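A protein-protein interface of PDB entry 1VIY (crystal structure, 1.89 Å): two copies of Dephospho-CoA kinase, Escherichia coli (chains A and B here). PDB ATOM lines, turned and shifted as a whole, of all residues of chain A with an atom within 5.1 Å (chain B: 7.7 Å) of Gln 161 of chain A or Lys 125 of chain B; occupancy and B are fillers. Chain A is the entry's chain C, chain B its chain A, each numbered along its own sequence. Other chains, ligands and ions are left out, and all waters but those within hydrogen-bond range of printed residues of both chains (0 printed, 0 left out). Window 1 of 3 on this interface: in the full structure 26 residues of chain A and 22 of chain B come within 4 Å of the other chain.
O of Lys 124 of chain B lies within hydrogen-bond range of N of Thr 163 of chain A, 3.2 Å away.
The backbone carbonyl oxygen (O) of Ala 126 of chain B is in hydrogen-bond range of the side-chain hydroxyl (OG1) of Thr 163 of chain A (2.8 Å).
The side-chain amide oxygen (OE1) of Gln 161 of chain A lies within hydrogen-bond range of the backbone NH (N) of Ile 13 of chain A (2.9 Å).
N of Ile 6 of chain B is in hydrogen-bond range of OD1 of Asn 127 of chain B (2.8 Å).
The side-chain carboxylate of Glu 119 of chain A sits at hydrogen-bond distance from the backbone NH of Ala 162 of chain A.
NH1 of Arg 167 of chain A is in hydrogen-bond range of O of Ala 162 of chain A (3.0 Å).
NE2 of Gln 95 of chain B lies close to NZ of Lys 125 of chain B (3.3 Å).
OE1 of Gln 99 of chain B lies within hydrogen-bond range of NZ of Lys 125 of chain B (3.4 Å).
Gln 99 of chain B touches Ala 159 of chain A (CD to O, 3.3 Å).
Ala 159 of chain A touches Lys 125 of chain B (O to NZ, 3.6 Å).
Ala 160 of chain A touches Gln 99 of chain B.
Ala 160 of chain A touches Lys 125 of chain B (O to NZ, 3.7 Å).
Lys 125 of chain B touches Gln 161 of chain A (CE to O, 3.7 Å).
O of Lys 124 of chain B touches CA of Ala 162 of chain A, at 3.4 Å.
Thr 163 of chain A touches Lys 125 of chain B (CG2 to C, 3.6 Å).
ND2 of Asn 127 of chain B touches CB of Thr 163 of chain A (3.8 Å).
Of chain B, only Lys 125 comes within 4 Å of Gln 161 of chain A.
Lys 125 of chain B touches just these residues of chain A: Ala 159, Ala 160, Gln 161 and Thr 163.
Ala 160 of chain A touches two residues of chain B.
Of the printed residues of chain B, Ala 162 of chain A touches Lys 124 (3.4 Å).
Of the printed residues of chain A, Gln 99 of chain B touches Ala 159 and Ala 160.
Printed residues of chain A within 4 Å of Lys 124 of chain B: Ala 162 and Thr 163.
The nearest residue of chain A that does not touch Lys 125 of chain B is Ala 162 of chain A (4.5 Å).
The nearest printed residue of chain B that does not touch Ala 162 of chain A is Lys 125 of chain B (4.5 Å).
Of the 20 printed residues of chain B, 5 touch a printed residue of chain A.
Hydrophobic or aromatic side chains of chain A within 4 Å of the printed part of chain B: Ala 159, Ala 160 and Ala 162.
Among the printed residues, no Asp or Glu carboxylate lies within 4 Å of a Lys or Arg side-chain nitrogen of the other chain.
No position is printed for both chains.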
ATOM      1  N   GLY A  12     -13.266  33.451  14.820  1.00  0.00           N
ATOM      2  CA  GLY A  12     -12.051  32.845  15.335  1.00  0.00           C
ATOM      3  C   GLY A  12     -10.980  32.775  14.270  1.00  0.00           C
ATOM      4  O   GLY A  12     -11.217  33.142  13.110  1.00  0.00           O
ATOM      5  N   ILE A  13      -9.798  32.300  14.656  1.00  0.00           N
ATOM      6  CA  ILE A  13      -8.702  32.221  13.673  1.00  0.00           C
ATOM      7  C   ILE A  13      -9.103  31.312  12.505  1.00  0.00           C
ATOM      8  O   ILE A  13      -9.765  30.293  12.692  1.00  0.00           O
ATOM      9  CB  ILE A  13      -7.388  31.741  14.323  1.00  0.00           C
ATOM     10  CG1 ILE A  13      -6.235  31.736  13.277  1.00  0.00           C
ATOM     11  CG2 ILE A  13      -7.542  30.341  14.950  1.00  0.00           C
ATOM     12  CD1 ILE A  13      -4.888  31.685  13.921  1.00  0.00           C
ATOM     13  N   GLU A 119     -13.953  38.168  23.936  1.00  0.00           N
ATOM     14  CA  GLU A 119     -13.028  38.089  25.056  1.00  0.00           C
ATOM     15  C   GLU A 119     -12.917  39.403  25.828  1.00  0.00           C
ATOM     16  O   GLU A 119     -12.830  39.408  27.057  1.00  0.00           O
ATOM     17  CB  GLU A 119     -11.648  37.672  24.539  1.00  0.00           C
ATOM     18  CG  GLU A 119     -11.575  36.236  24.021  1.00  0.00           C
ATOM     19  CD  GLU A 119     -11.786  36.152  22.531  1.00  0.00           C
ATOM     20  OE1 GLU A 119     -12.504  37.000  21.946  1.00  0.00           O
ATOM     21  OE2 GLU A 119     -11.260  35.198  21.949  1.00  0.00           O
ATOM     22  N   GLN A 139     -11.320  26.034  10.556  1.00  0.00           N
ATOM     23  CA  GLN A 139     -10.304  26.873  11.219  1.00  0.00           C
ATOM     24  C   GLN A 139      -8.901  26.239  11.215  1.00  0.00           C
ATOM     25  O   GLN A 139      -7.870  26.909  10.906  1.00  0.00           O
ATOM     26  CB  GLN A 139     -10.694  27.116  12.694  1.00  0.00           C
ATOM     27  CG  GLN A 139     -12.024  27.861  12.902  1.00  0.00           C
ATOM     28  CD  GLN A 139     -12.217  28.190  14.360  1.00  0.00           C
ATOM     29  OE1 GLN A 139     -12.995  27.519  15.052  1.00  0.00           O
ATOM     30  NE2 GLN A 139     -11.476  29.200  14.848  1.00  0.00           N
ATOM     31  N   ILE A 157      -4.059  27.280  19.621  1.00  0.00           N
ATOM     32  CA  ILE A 157      -4.649  28.612  19.428  1.00  0.00           C
ATOM     33  C   ILE A 157      -6.191  28.557  19.629  1.00  0.00           C
ATOM     34  O   ILE A 157      -6.770  29.399  20.316  1.00  0.00           O
ATOM     35  CB  ILE A 157      -4.277  29.244  18.041  1.00  0.00           C
ATOM     36  CG1 ILE A 157      -2.746  29.360  17.873  1.00  0.00           C
ATOM     37  CG2 ILE A 157      -4.952  30.625  17.894  1.00  0.00           C
ATOM     38  CD1 ILE A 157      -2.261  29.844  16.477  1.00  0.00           C
ATOM     39  N   LEU A 158      -6.842  27.569  19.033  1.00  0.00           N
ATOM     40  CA  LEU A 158      -8.297  27.391  19.191  1.00  0.00           C
ATOM     41  C   LEU A 158      -8.704  27.286  20.672  1.00  0.00           C
ATOM     42  O   LEU A 158      -9.664  27.933  21.119  1.00  0.00           O
ATOM     43  CB  LEU A 158      -8.774  26.149  18.436  1.00  0.00           C
ATOM     44  CG  LEU A 158      -8.881  26.198  16.909  1.00  0.00           C
ATOM     45  CD1 LEU A 158      -9.837  25.106  16.422  1.00  0.00           C
ATOM     46  CD2 LEU A 158      -9.361  27.544  16.400  1.00  0.00           C
ATOM     47  N   ALA A 159      -7.950  26.485  21.422  1.00  0.00           N
ATOM     48  CA  ALA A 159      -8.152  26.356  22.866  1.00  0.00           C
ATOM     49  C   ALA A 159      -7.975  27.650  23.649  1.00  0.00           C
ATOM     50  O   ALA A 159      -8.549  27.785  24.732  1.00  0.00           O
ATOM     51  CB  ALA A 159      -7.248  25.243  23.435  1.00  0.00           C
ATOM     52  N   ALA A 160      -7.206  28.611  23.120  1.00  0.00           N
ATOM     53  CA  ALA A 160      -7.043  29.886  23.797  1.00  0.00           C
ATOM     54  C   ALA A 160      -8.082  30.956  23.454  1.00  0.00           C
ATOM     55  O   ALA A 160      -8.271  31.882  24.219  1.00  0.00           O
ATOM     56  CB  ALA A 160      -5.629  30.439  23.598  1.00  0.00           C
ATOM     57  N   GLN A 161      -8.749  30.852  22.308  1.00  0.00           N
ATOM     58  CA  GLN A 161      -9.713  31.896  21.946  1.00  0.00           C
ATOM     59  C   GLN A 161     -11.079  31.498  22.538  1.00  0.00           C
ATOM     60  O   GLN A 161     -11.264  30.370  22.941  1.00  0.00           O
ATOM     61  CB  GLN A 161      -9.816  32.017  20.424  1.00  0.00           C
ATOM     62  CG  GLN A 161      -8.508  32.347  19.717  1.00  0.00           C
ATOM     63  CD  GLN A 161      -8.696  32.598  18.222  1.00  0.00           C
ATOM     64  OE1 GLN A 161      -9.482  31.903  17.549  1.00  0.00           O
ATOM     65  NE2 GLN A 161      -7.961  33.595  17.687  1.00  0.00           N
ATOM     66  N   ALA A 162     -12.023  32.432  22.576  1.00  0.00           N
ATOM     67  CA  ALA A 162     -13.392  32.134  22.910  1.00  0.00           C
ATOM     68  C   ALA A 162     -13.917  31.018  21.999  1.00  0.00           C
ATOM     69  O   ALA A 162     -13.455  30.871  20.869  1.00  0.00           O
ATOM     70  CB  ALA A 162     -14.239  33.412  22.765  1.00  0.00           C
ATOM     71  N   THR A 163     -14.856  30.213  22.501  1.00  0.00           N
ATOM     72  CA  THR A 163     -15.424  29.128  21.711  1.00  0.00           C
ATOM     73  C   THR A 163     -16.351  29.640  20.622  1.00  0.00           C
ATOM     74  O   THR A 163     -16.804  30.783  20.673  1.00  0.00           O
ATOM     75  CB  THR A 163     -16.196  28.163  22.597  1.00  0.00           C
ATOM     76  OG1 THR A 163     -17.291  28.868  23.199  1.00  0.00           O
ATOM     77  CG2 THR A 163     -15.264  27.711  23.787  1.00  0.00           C
ATOM     78  N   ARG A 167     -19.194  32.901  20.661  1.00  0.00           N
ATOM     79  CA  ARG A 167     -19.384  33.944  19.647  1.00  0.00           C
ATOM     80  C   ARG A 167     -20.838  33.985  19.197  1.00  0.00           C
ATOM     81  O   ARG A 167     -21.463  35.059  19.117  1.00  0.00           O
ATOM     82  CB  ARG A 167     -18.438  33.787  18.472  1.00  0.00           C
ATOM     83  CG  ARG A 167     -16.949  33.975  18.808  1.00  0.00           C
ATOM     84  CD  ARG A 167     -16.083  34.025  17.547  1.00  0.00           C
ATOM     85  NE  ARG A 167     -15.949  32.678  16.993  1.00  0.00           N
ATOM     86  CZ  ARG A 167     -14.980  31.806  17.318  1.00  0.00           C
ATOM     87  NH1 ARG A 167     -14.055  32.125  18.194  1.00  0.00           N
ATOM     88  NH2 ARG A 167     -14.949  30.607  16.759  1.00  0.00           N
ATOM     89  N   ILE B   6     -16.019  20.897  25.734  1.00  0.00           N
ATOM     90  CA  ILE B   6     -16.037  21.400  27.111  1.00  0.00           C
ATOM     91  C   ILE B   6     -17.459  21.767  27.545  1.00  0.00           C
ATOM     92  O   ILE B   6     -18.067  22.730  27.018  1.00  0.00           O
ATOM     93  CB  ILE B   6     -15.107  22.660  27.278  1.00  0.00           C
ATOM     94  CG1 ILE B   6     -13.640  22.357  26.906  1.00  0.00           C
ATOM     95  CG2 ILE B   6     -15.154  23.237  28.701  1.00  0.00           C
ATOM     96  CD1 ILE B   6     -12.857  23.644  26.587  1.00  0.00           C
ATOM     97  N   VAL B   7     -17.989  20.999  28.496  1.00  0.00           N
ATOM     98  CA  VAL B   7     -19.225  21.367  29.190  1.00  0.00           C
ATOM     99  C   VAL B   7     -18.856  22.012  30.549  1.00  0.00           C
ATOM    100  O   VAL B   7     -18.319  21.337  31.429  1.00  0.00           O
ATOM    101  CB  VAL B   7     -20.176  20.142  29.383  1.00  0.00           C
ATOM    102  CG1 VAL B   7     -21.527  20.564  30.008  1.00  0.00           C
ATOM    103  CG2 VAL B   7     -20.480  19.515  28.041  1.00  0.00           C
ATOM    104  N   ALA B   8     -19.159  23.300  30.713  1.00  0.00           N
ATOM    105  CA  ALA B   8     -19.015  23.948  32.037  1.00  0.00           C
ATOM    106  C   ALA B   8     -20.180  23.643  32.991  1.00  0.00           C
ATOM    107  O   ALA B   8     -21.321  23.692  32.589  1.00  0.00           O
ATOM    108  CB  ALA B   8     -18.875  25.443  31.859  1.00  0.00           C
ATOM    109  N   HIS B  91      -5.421  34.690  36.889  1.00  0.00           N
ATOM    110  CA  HIS B  91      -6.425  34.528  35.821  1.00  0.00           C
ATOM    111  C   HIS B  91      -5.827  33.810  34.601  1.00  0.00           C
ATOM    112  O   HIS B  91      -6.261  32.706  34.303  1.00  0.00           O
ATOM    113  CB  HIS B  91      -7.143  35.837  35.431  1.00  0.00           C
ATOM    114  CG  HIS B  91      -7.910  35.734  34.142  1.00  0.00           C
ATOM    115  ND1 HIS B  91      -7.348  36.013  32.913  1.00  0.00           N
ATOM    116  CD2 HIS B  91      -9.182  35.326  33.887  1.00  0.00           C
ATOM    117  CE1 HIS B  91      -8.240  35.807  31.961  1.00  0.00           C
ATOM    118  NE2 HIS B  91      -9.364  35.393  32.523  1.00  0.00           N
ATOM    119  N   GLN B  95      -6.271  29.667  33.486  1.00  0.00           N
ATOM    120  CA  GLN B  95      -6.752  29.245  32.144  1.00  0.00           C
ATOM    121  C   GLN B  95      -5.777  28.334  31.383  1.00  0.00           C
ATOM    122  O   GLN B  95      -6.209  27.334  30.769  1.00  0.00           O
ATOM    123  CB  GLN B  95      -7.145  30.457  31.286  1.00  0.00           C
ATOM    124  CG  GLN B  95      -8.111  30.141  30.119  1.00  0.00           C
ATOM    125  CD  GLN B  95      -9.357  29.290  30.508  1.00  0.00           C
ATOM    126  OE1 GLN B  95     -10.224  29.713  31.317  1.00  0.00           O
ATOM    127  NE2 GLN B  95      -9.447  28.108  29.920  1.00  0.00           N
ATOM    128  N   GLN B  96      -4.481  28.673  31.417  1.00  0.00           N
ATOM    129  CA  GLN B  96      -3.448  27.865  30.754  1.00  0.00           C
ATOM    130  C   GLN B  96      -3.353  26.461  31.330  1.00  0.00           C
ATOM    131  O   GLN B  96      -3.363  25.467  30.558  1.00  0.00           O
ATOM    132  CB  GLN B  96      -2.068  28.570  30.719  1.00  0.00           C
ATOM    133  CG  GLN B  96      -2.065  29.832  29.845  1.00  0.00           C
ATOM    134  CD  GLN B  96      -1.005  30.893  30.238  1.00  0.00           C
ATOM    135  OE1 GLN B  96       0.081  30.578  30.750  1.00  0.00           O
ATOM    136  NE2 GLN B  96      -1.342  32.162  29.993  1.00  0.00           N
ATOM    137  N   THR B  98      -5.811  24.944  32.970  1.00  0.00           N
ATOM    138  CA  THR B  98      -7.094  24.353  32.552  1.00  0.00           C
ATOM    139  C   THR B  98      -7.016  23.770  31.119  1.00  0.00           C
ATOM    140  O   THR B  98      -7.340  22.603  30.889  1.00  0.00           O
ATOM    141  CB  THR B  98      -8.219  25.434  32.670  1.00  0.00           C
ATOM    142  OG1 THR B  98      -8.326  25.889  34.041  1.00  0.00           O
ATOM    143  CG2 THR B  98      -9.624  24.823  32.347  1.00  0.00           C
ATOM    144  N   GLN B  99      -6.581  24.589  30.169  1.00  0.00           N
ATOM    145  CA  GLN B  99      -6.409  24.184  28.778  1.00  0.00           C
ATOM    146  C   GLN B  99      -5.516  22.953  28.701  1.00  0.00           C
ATOM    147  O   GLN B  99      -5.821  21.992  27.981  1.00  0.00           O
ATOM    148  CB  GLN B  99      -5.791  25.327  27.942  1.00  0.00           C
ATOM    149  CG  GLN B  99      -6.791  26.380  27.418  1.00  0.00           C
ATOM    150  CD  GLN B  99      -6.092  27.692  26.930  1.00  0.00           C
ATOM    151  OE1 GLN B  99      -6.347  28.792  27.450  1.00  0.00           O
ATOM    152  NE2 GLN B  99      -5.213  27.557  25.950  1.00  0.00           N
ATOM    153  N   ILE B 102      -7.443  19.905  30.044  1.00  0.00           N
ATOM    154  CA  ILE B 102      -8.510  19.500  29.110  1.00  0.00           C
ATOM    155  C   ILE B 102      -7.853  18.763  27.923  1.00  0.00           C
ATOM    156  O   ILE B 102      -8.258  17.652  27.556  1.00  0.00           O
ATOM    157  CB  ILE B 102      -9.349  20.732  28.672  1.00  0.00           C
ATOM    158  CG1 ILE B 102     -10.172  21.258  29.871  1.00  0.00           C
ATOM    159  CG2 ILE B 102     -10.194  20.432  27.374  1.00  0.00           C
ATOM    160  CD1 ILE B 102     -10.806  22.649  29.660  1.00  0.00           C
ATOM    161  N   TRP B 112     -16.280  20.700  33.233  1.00  0.00           N
ATOM    162  CA  TRP B 112     -15.426  21.711  33.832  1.00  0.00           C
ATOM    163  C   TRP B 112     -16.220  22.437  34.900  1.00  0.00           C
ATOM    164  O   TRP B 112     -17.160  23.163  34.591  1.00  0.00           O
ATOM    165  CB  TRP B 112     -14.907  22.680  32.715  1.00  0.00           C
ATOM    166  CG  TRP B 112     -14.105  23.828  33.154  1.00  0.00           C
ATOM    167  CD1 TRP B 112     -13.163  23.864  34.181  1.00  0.00           C
ATOM    168  CD2 TRP B 112     -14.083  25.130  32.556  1.00  0.00           C
ATOM    169  NE1 TRP B 112     -12.586  25.100  34.247  1.00  0.00           N
ATOM    170  CE2 TRP B 112     -13.130  25.907  33.274  1.00  0.00           C
ATOM    171  CE3 TRP B 112     -14.804  25.739  31.523  1.00  0.00           C
ATOM    172  CZ2 TRP B 112     -12.856  27.253  32.968  1.00  0.00           C
ATOM    173  CZ3 TRP B 112     -14.521  27.108  31.193  1.00  0.00           C
ATOM    174  CH2 TRP B 112     -13.540  27.831  31.907  1.00  0.00           C
ATOM    175  N   LEU B 117     -18.273  30.766  37.360  1.00  0.00           N
ATOM    176  CA  LEU B 117     -18.457  30.794  35.889  1.00  0.00           C
ATOM    177  C   LEU B 117     -19.143  32.079  35.462  1.00  0.00           C
ATOM    178  O   LEU B 117     -18.634  32.777  34.600  1.00  0.00           O
ATOM    179  CB  LEU B 117     -19.296  29.598  35.409  1.00  0.00           C
ATOM    180  CG  LEU B 117     -19.348  29.356  33.886  1.00  0.00           C
ATOM    181  CD1 LEU B 117     -18.033  28.756  33.355  1.00  0.00           C
ATOM    182  CD2 LEU B 117     -20.570  28.443  33.546  1.00  0.00           C
ATOM    183  N   SER B 121     -17.422  35.529  34.018  1.00  0.00           N
ATOM    184  CA  SER B 121     -17.698  35.329  32.563  1.00  0.00           C
ATOM    185  C   SER B 121     -16.855  34.220  31.894  1.00  0.00           C
ATOM    186  O   SER B 121     -16.479  34.309  30.710  1.00  0.00           O
ATOM    187  CB  SER B 121     -17.526  36.631  31.776  1.00  0.00           C
ATOM    188  OG  SER B 121     -18.298  37.665  32.390  1.00  0.00           O
ATOM    189  N   LEU B 122     -16.591  33.166  32.638  1.00  0.00           N
ATOM    190  CA  LEU B 122     -15.747  32.112  32.122  1.00  0.00           C
ATOM    191  C   LEU B 122     -16.490  31.153  31.184  1.00  0.00           C
ATOM    192  O   LEU B 122     -15.870  30.228  30.615  1.00  0.00           O
ATOM    193  CB  LEU B 122     -15.100  31.373  33.292  1.00  0.00           C
ATOM    194  CG  LEU B 122     -14.000  32.125  34.029  1.00  0.00           C
ATOM    195  CD1 LEU B 122     -13.719  31.505  35.425  1.00  0.00           C
ATOM    196  CD2 LEU B 122     -12.697  32.304  33.170  1.00  0.00           C
ATOM    197  N   TYR B 123     -17.813  31.337  31.043  1.00  0.00           N
ATOM    198  CA  TYR B 123     -18.586  30.609  30.034  1.00  0.00           C
ATOM    199  C   TYR B 123     -18.118  30.870  28.595  1.00  0.00           C
ATOM    200  O   TYR B 123     -18.387  30.056  27.691  1.00  0.00           O
ATOM    201  CB  TYR B 123     -20.102  30.886  30.205  1.00  0.00           C
ATOM    202  CG  TYR B 123     -20.462  32.328  30.350  1.00  0.00           C
ATOM    203  CD1 TYR B 123     -20.372  33.218  29.264  1.00  0.00           C
ATOM    204  CD2 TYR B 123     -20.851  32.824  31.585  1.00  0.00           C
ATOM    205  CE1 TYR B 123     -20.675  34.573  29.426  1.00  0.00           C
ATOM    206  CE2 TYR B 123     -21.142  34.133  31.742  1.00  0.00           C
ATOM    207  CZ  TYR B 123     -21.062  34.999  30.666  1.00  0.00           C
ATOM    208  OH  TYR B 123     -21.387  36.293  30.885  1.00  0.00           O
ATOM    209  N   LYS B 124     -17.386  31.982  28.385  1.00  0.00           N
ATOM    210  CA  LYS B 124     -16.819  32.337  27.077  1.00  0.00           C
ATOM    211  C   LYS B 124     -15.799  31.268  26.670  1.00  0.00           C
ATOM    212  O   LYS B 124     -15.430  31.168  25.512  1.00  0.00           O
ATOM    213  CB  LYS B 124     -16.093  33.710  27.140  1.00  0.00           C
ATOM    214  CG  LYS B 124     -17.070  34.874  27.400  1.00  0.00           C
ATOM    215  CD  LYS B 124     -16.331  36.199  27.742  1.00  0.00           C
ATOM    216  CE  LYS B 124     -17.385  37.352  27.695  1.00  0.00           C
ATOM    217  NZ  LYS B 124     -16.687  38.623  27.797  1.00  0.00           N
ATOM    218  N   LYS B 125     -15.337  30.469  27.633  1.00  0.00           N
ATOM    219  CA  LYS B 125     -14.357  29.428  27.324  1.00  0.00           C
ATOM    220  C   LYS B 125     -14.956  28.021  27.339  1.00  0.00           C
ATOM    221  O   LYS B 125     -14.215  27.040  27.347  1.00  0.00           O
ATOM    222  CB  LYS B 125     -13.176  29.515  28.279  1.00  0.00           C
ATOM    223  CG  LYS B 125     -12.494  30.918  28.290  1.00  0.00           C
ATOM    224  CD  LYS B 125     -11.754  31.216  26.977  1.00  0.00           C
ATOM    225  CE  LYS B 125     -10.806  30.070  26.581  1.00  0.00           C
ATOM    226  NZ  LYS B 125      -9.462  30.131  27.260  1.00  0.00           N
ATOM    227  N   ALA B 126     -16.282  27.932  27.388  1.00  0.00           N
ATOM    228  CA  ALA B 126     -16.943  26.621  27.327  1.00  0.00           C
ATOM    229  C   ALA B 126     -17.698  26.471  26.032  1.00  0.00           C
ATOM    230  O   ALA B 126     -18.212  27.471  25.461  1.00  0.00           O
ATOM    231  CB  ALA B 126     -17.929  26.449  28.514  1.00  0.00           C
ATOM    232  N   ASN B 127     -17.807  25.225  25.578  1.00  0.00           N
ATOM    233  CA  ASN B 127     -18.653  24.921  24.423  1.00  0.00           C
ATOM    234  C   ASN B 127     -20.148  24.851  24.818  1.00  0.00           C
ATOM    235  O   ASN B 127     -20.987  25.109  23.995  1.00  0.00           O
ATOM    236  CB  ASN B 127     -18.214  23.572  23.816  1.00  0.00           C
ATOM    237  CG  ASN B 127     -16.803  23.609  23.327  1.00  0.00           C
ATOM    238  OD1 ASN B 127     -15.904  22.996  23.900  1.00  0.00           O
ATOM    239  ND2 ASN B 127     -16.575  24.414  22.305  1.00  0.00           N
ATOM    240  N   ARG B 128     -20.461  24.521  26.072  1.00  0.00           N
ATOM    241  CA  ARG B 128     -21.847  24.339  26.525  1.00  0.00           C
ATOM    242  C   ARG B 128     -21.898  24.612  28.047  1.00  0.00           C
ATOM    243  O   ARG B 128     -20.886  24.387  28.761  1.00  0.00           O
ATOM    244  CB  ARG B 128     -22.298  22.900  26.189  1.00  0.00           C
ATOM    245  CG  ARG B 128     -23.783  22.597  26.544  1.00  0.00           C
ATOM    246  CD  ARG B 128     -24.564  22.123  25.380  1.00  0.00           C
ATOM    247  NE  ARG B 128     -25.996  21.891  25.629  1.00  0.00           N
ATOM    248  CZ  ARG B 128     -26.904  22.150  24.716  1.00  0.00           C
ATOM    249  NH1 ARG B 128     -26.515  22.616  23.534  1.00  0.00           N
ATOM    250  NH2 ARG B 128     -28.190  21.913  24.963  1.00  0.00           N
ATOM    251  N   VAL B 129     -23.020  25.137  28.552  1.00  0.00           N
ATOM    252  CA  VAL B 129     -23.119  25.520  29.985  1.00  0.00           C
ATOM    253  C   VAL B 129     -24.265  24.750  30.623  1.00  0.00           C
ATOM    254  O   VAL B 129     -25.421  24.790  30.152  1.00  0.00           O
ATOM    255  CB  VAL B 129     -23.321  27.052  30.215  1.00  0.00           C
ATOM    256  CG1 VAL B 129     -23.515  27.391  31.738  1.00  0.00           C
ATOM    257  CG2 VAL B 129     -22.116  27.865  29.643  1.00  0.00           C
